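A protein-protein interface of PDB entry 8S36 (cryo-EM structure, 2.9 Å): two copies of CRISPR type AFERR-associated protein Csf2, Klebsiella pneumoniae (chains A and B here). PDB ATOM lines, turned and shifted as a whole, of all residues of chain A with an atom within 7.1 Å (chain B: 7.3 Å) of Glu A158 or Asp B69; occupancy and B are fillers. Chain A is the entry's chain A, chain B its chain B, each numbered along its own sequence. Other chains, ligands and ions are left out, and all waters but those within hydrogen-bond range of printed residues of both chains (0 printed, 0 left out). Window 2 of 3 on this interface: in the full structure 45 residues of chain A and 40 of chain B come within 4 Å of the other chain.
O of Gly B70 lies close to O of Glu A158.
O of Phe A159 sits at hydrogen-bond distance from OG of Ser B72 (2.6 Å).
O of Leu A160 lies within hydrogen-bond range of NZ of Lys B71 (3.0 Å).
OE2 of Glu A158 sits close to O of Asp B69, 3.2 Å away.
Glu A158 touches just these residues of chain B: Asp B69, Gly B70 and Lys B71.
Of chain A, only Glu A158 comes within 4 Å of Asp B69.
Printed residues of chain A within 4 Å of Leu B66: Phe A159 (3.4 Å).
Of the printed residues of chain A, Ser B72 touches Phe A159 (2.6 Å).
Of the printed residues of chain B, Glu A161 touches Lys B71.
Asn B67 touches none of the printed residues of chain A.
The nearest printed residue of chain B that does not touch Glu A158 is Leu B66 (5.2 Å).
The nearest residue of chain A that does not touch Asp B69 is Glu A161 (6.7 Å).
Hydrophobic or aromatic side chains of chain A within 4 Å of the printed part of chain B: Phe A159.
Of the 7 printed residues of chain B, 5 touch a printed residue of chain A.
Printed residues of chain B that touch a printed residue of chain A: Leu B66, Asp B69, Gly B70, Lys B71 and Ser B72.
Hydrophobic or aromatic side chains of chain B within 4 Å of the printed part of chain A: Leu B66.
Among the printed residues, no Asp or Glu carboxylate lies within 4 Å of a Lys or Arg side-chain nitrogen of the other chain.
O of Glu A158 touches CD of Lys B71, 3.8 Å away.
Leu B66 touches Phe A159 (CD1 to CD1, 3.4 Å).
Gly B70 touches Phe A159.
Phe A159 touches Lys B71.
CA of Glu A161 touches NZ of Lys B71, at 3.5 Å.
The side-chain amide oxygen (OD1) of Asn B67 sits close to the backbone carbonyl oxygen (O) of Lys B71 (2.6 Å).
No position is printed for both chains.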
ATOM      1  N   PHE A 150      12.688  22.698  12.077  1.00  0.00           N
ATOM      2  CA  PHE A 150      12.137  22.042  10.901  1.00  0.00           C
ATOM      3  C   PHE A 150      12.250  22.885   9.642  1.00  0.00           C
ATOM      4  O   PHE A 150      12.168  22.335   8.538  1.00  0.00           O
ATOM      5  CB  PHE A 150      10.677  21.665  11.156  1.00  0.00           C
ATOM      6  CG  PHE A 150      10.496  20.757  12.336  1.00  0.00           C
ATOM      7  CD1 PHE A 150      10.941  19.447  12.290  1.00  0.00           C
ATOM      8  CD2 PHE A 150       9.889  21.211  13.493  1.00  0.00           C
ATOM      9  CE1 PHE A 150      10.785  18.608  13.375  1.00  0.00           C
ATOM     10  CE2 PHE A 150       9.733  20.377  14.581  1.00  0.00           C
ATOM     11  CZ  PHE A 150      10.179  19.073  14.521  1.00  0.00           C
ATOM     12  N   GLU A 154      15.268  19.359   6.898  1.00  0.00           N
ATOM     13  CA  GLU A 154      14.076  18.622   6.504  1.00  0.00           C
ATOM     14  C   GLU A 154      14.127  17.158   6.914  1.00  0.00           C
ATOM     15  O   GLU A 154      13.077  16.507   6.968  1.00  0.00           O
ATOM     16  CB  GLU A 154      13.874  18.721   4.990  1.00  0.00           C
ATOM     17  CG  GLU A 154      13.447  20.103   4.522  1.00  0.00           C
ATOM     18  CD  GLU A 154      13.155  20.153   3.036  1.00  0.00           C
ATOM     19  OE1 GLU A 154      13.346  19.123   2.357  1.00  0.00           O
ATOM     20  OE2 GLU A 154      12.735  21.223   2.548  1.00  0.00           O
ATOM     21  N   SER A 155      15.320  16.625   7.199  1.00  0.00           N
ATOM     22  CA  SER A 155      15.422  15.275   7.743  1.00  0.00           C
ATOM     23  C   SER A 155      14.595  15.118   9.013  1.00  0.00           C
ATOM     24  O   SER A 155      14.121  14.016   9.312  1.00  0.00           O
ATOM     25  CB  SER A 155      16.884  14.924   8.018  1.00  0.00           C
ATOM     26  OG  SER A 155      16.984  13.790   8.861  1.00  0.00           O
ATOM     27  N   LEU A 156      14.411  16.200   9.768  1.00  0.00           N
ATOM     28  CA  LEU A 156      13.662  16.152  11.016  1.00  0.00           C
ATOM     29  C   LEU A 156      12.155  16.148  10.802  1.00  0.00           C
ATOM     30  O   LEU A 156      11.410  16.045  11.783  1.00  0.00           O
ATOM     31  CB  LEU A 156      14.047  17.337  11.905  1.00  0.00           C
ATOM     32  CG  LEU A 156      15.492  17.339  12.407  1.00  0.00           C
ATOM     33  CD1 LEU A 156      15.899  18.718  12.901  1.00  0.00           C
ATOM     34  CD2 LEU A 156      15.667  16.301  13.505  1.00  0.00           C
ATOM     35  N   MET A 157      11.689  16.247   9.557  1.00  0.00           N
ATOM     36  CA  MET A 157      10.270  16.151   9.246  1.00  0.00           C
ATOM     37  C   MET A 157       9.853  14.757   8.806  1.00  0.00           C
ATOM     38  O   MET A 157       8.657  14.521   8.604  1.00  0.00           O
ATOM     39  CB  MET A 157       9.889  17.151   8.153  1.00  0.00           C
ATOM     40  CG  MET A 157      10.053  18.608   8.559  1.00  0.00           C
ATOM     41  SD  MET A 157       8.548  19.361   9.231  1.00  0.00           S
ATOM     42  CE  MET A 157       7.323  19.068   7.953  1.00  0.00           C
ATOM     43  N   GLU A 158      10.799  13.834   8.654  1.00  0.00           N
ATOM     44  CA  GLU A 158      10.466  12.435   8.435  1.00  0.00           C
ATOM     45  C   GLU A 158      10.174  11.702   9.736  1.00  0.00           C
ATOM     46  O   GLU A 158       9.922  10.493   9.704  1.00  0.00           O
ATOM     47  CB  GLU A 158      11.608  11.737   7.689  1.00  0.00           C
ATOM     48  CG  GLU A 158      11.184  10.501   6.902  1.00  0.00           C
ATOM     49  CD  GLU A 158      11.547   9.200   7.595  1.00  0.00           C
ATOM     50  OE1 GLU A 158      12.662   9.102   8.149  1.00  0.00           O
ATOM     51  OE2 GLU A 158      10.711   8.273   7.585  1.00  0.00           O
ATOM     52  N   PHE A 159      10.192  12.406  10.871  1.00  0.00           N
ATOM     53  CA  PHE A 159       9.971  11.807  12.182  1.00  0.00           C
ATOM     54  C   PHE A 159       8.722  12.350  12.864  1.00  0.00           C
ATOM     55  O   PHE A 159       8.500  12.056  14.044  1.00  0.00           O
ATOM     56  CB  PHE A 159      11.186  12.047  13.084  1.00  0.00           C
ATOM     57  CG  PHE A 159      12.506  11.832  12.402  1.00  0.00           C
ATOM     58  CD1 PHE A 159      12.714  10.736  11.584  1.00  0.00           C
ATOM     59  CD2 PHE A 159      13.542  12.733  12.581  1.00  0.00           C
ATOM     60  CE1 PHE A 159      13.930  10.540  10.959  1.00  0.00           C
ATOM     61  CE2 PHE A 159      14.759  12.544  11.958  1.00  0.00           C
ATOM     62  CZ  PHE A 159      14.954  11.447  11.146  1.00  0.00           C
ATOM     63  N   LEU A 160       7.903  13.128  12.159  1.00  0.00           N
ATOM     64  CA  LEU A 160       6.691  13.717  12.710  1.00  0.00           C
ATOM     65  C   LEU A 160       5.486  13.171  11.962  1.00  0.00           C
ATOM     66  O   LEU A 160       5.498  13.101  10.728  1.00  0.00           O
ATOM     67  CB  LEU A 160       6.723  15.242  12.602  1.00  0.00           C
ATOM     68  CG  LEU A 160       7.222  16.004  13.828  1.00  0.00           C
ATOM     69  CD1 LEU A 160       8.680  15.682  14.111  1.00  0.00           C
ATOM     70  CD2 LEU A 160       7.027  17.495  13.623  1.00  0.00           C
ATOM     71  N   GLU A 161       4.452  12.790  12.703  1.00  0.00           N
ATOM     72  CA  GLU A 161       3.209  12.385  12.071  1.00  0.00           C
ATOM     73  C   GLU A 161       2.484  13.608  11.516  1.00  0.00           C
ATOM     74  O   GLU A 161       2.769  14.751  11.881  1.00  0.00           O
ATOM     75  CB  GLU A 161       2.322  11.641  13.069  1.00  0.00           C
ATOM     76  CG  GLU A 161       2.886  10.299  13.509  1.00  0.00           C
ATOM     77  CD  GLU A 161       2.093   9.671  14.637  1.00  0.00           C
ATOM     78  OE1 GLU A 161       1.298  10.388  15.280  1.00  0.00           O
ATOM     79  OE2 GLU A 161       2.268   8.459  14.882  1.00  0.00           O
ATOM     80  N   VAL A 165       2.649  17.601  11.896  1.00  0.00           N
ATOM     81  CA  VAL A 165       3.065  18.514  10.841  1.00  0.00           C
ATOM     82  C   VAL A 165       2.025  19.605  10.657  1.00  0.00           C
ATOM     83  O   VAL A 165       2.365  20.738  10.286  1.00  0.00           O
ATOM     84  CB  VAL A 165       3.304  17.745   9.528  1.00  0.00           C
ATOM     85  CG1 VAL A 165       3.589  18.708   8.387  1.00  0.00           C
ATOM     86  CG2 VAL A 165       4.450  16.756   9.696  1.00  0.00           C
ATOM     87  N   LEU B  66      12.342   4.549  15.739  1.00  0.00           N
ATOM     88  CA  LEU B  66      11.489   5.046  14.663  1.00  0.00           C
ATOM     89  C   LEU B  66      10.446   3.980  14.357  1.00  0.00           C
ATOM     90  O   LEU B  66      10.721   3.017  13.637  1.00  0.00           O
ATOM     91  CB  LEU B  66      12.322   5.381  13.429  1.00  0.00           C
ATOM     92  CG  LEU B  66      13.219   6.628  13.451  1.00  0.00           C
ATOM     93  CD1 LEU B  66      12.396   7.906  13.441  1.00  0.00           C
ATOM     94  CD2 LEU B  66      14.183   6.627  14.632  1.00  0.00           C
ATOM     95  N   ASN B  67       9.241   4.142  14.897  1.00  0.00           N
ATOM     96  CA  ASN B  67       8.163   3.204  14.627  1.00  0.00           C
ATOM     97  C   ASN B  67       7.373   3.690  13.411  1.00  0.00           C
ATOM     98  O   ASN B  67       7.764   4.641  12.732  1.00  0.00           O
ATOM     99  CB  ASN B  67       7.288   3.023  15.870  1.00  0.00           C
ATOM    100  CG  ASN B  67       6.581   4.299  16.290  1.00  0.00           C
ATOM    101  OD1 ASN B  67       6.711   5.340  15.650  1.00  0.00           O
ATOM    102  ND2 ASN B  67       5.826   4.220  17.378  1.00  0.00           N
ATOM    103  N   ALA B  68       6.238   3.044  13.136  1.00  0.00           N
ATOM    104  CA  ALA B  68       5.435   3.364  11.963  1.00  0.00           C
ATOM    105  C   ALA B  68       6.298   3.274  10.707  1.00  0.00           C
ATOM    106  O   ALA B  68       7.085   2.332  10.567  1.00  0.00           O
ATOM    107  CB  ALA B  68       4.805   4.751  12.121  1.00  0.00           C
ATOM    108  N   ASP B  69       6.169   4.236   9.788  1.00  0.00           N
ATOM    109  CA  ASP B  69       7.012   4.309   8.601  1.00  0.00           C
ATOM    110  C   ASP B  69       8.151   5.310   8.768  1.00  0.00           C
ATOM    111  O   ASP B  69       8.588   5.925   7.789  1.00  0.00           O
ATOM    112  CB  ASP B  69       6.170   4.666   7.375  1.00  0.00           C
ATOM    113  CG  ASP B  69       5.510   6.026   7.493  1.00  0.00           C
ATOM    114  OD1 ASP B  69       5.501   6.590   8.607  1.00  0.00           O
ATOM    115  OD2 ASP B  69       5.000   6.531   6.471  1.00  0.00           O
ATOM    116  N   GLY B  70       8.638   5.485   9.997  1.00  0.00           N
ATOM    117  CA  GLY B  70       9.695   6.429  10.299  1.00  0.00           C
ATOM    118  C   GLY B  70       9.271   7.596  11.163  1.00  0.00           C
ATOM    119  O   GLY B  70      10.093   8.483  11.420  1.00  0.00           O
ATOM    120  N   LYS B  71       8.020   7.635  11.613  1.00  0.00           N
ATOM    121  CA  LYS B  71       7.562   8.683  12.514  1.00  0.00           C
ATOM    122  C   LYS B  71       8.023   8.377  13.933  1.00  0.00           C
ATOM    123  O   LYS B  71       7.861   7.255  14.418  1.00  0.00           O
ATOM    124  CB  LYS B  71       6.041   8.806  12.461  1.00  0.00           C
ATOM    125  CG  LYS B  71       5.460   8.856  11.051  1.00  0.00           C
ATOM    126  CD  LYS B  71       6.225   9.814  10.145  1.00  0.00           C
ATOM    127  CE  LYS B  71       5.485  10.063   8.841  1.00  0.00           C
ATOM    128  NZ  LYS B  71       4.276  10.909   9.029  1.00  0.00           N
ATOM    129  N   SER B  72       8.609   9.372  14.592  1.00  0.00           N
ATOM    130  CA  SER B  72       9.121   9.164  15.939  1.00  0.00           C
ATOM    131  C   SER B  72       7.998   9.349  16.962  1.00  0.00           C
ATOM    132  O   SER B  72       7.138  10.215  16.780  1.00  0.00           O
ATOM    133  CB  SER B  72      10.257  10.137  16.242  1.00  0.00           C
ATOM    134  OG  SER B  72       9.802  11.479  16.202  1.00  0.00           O
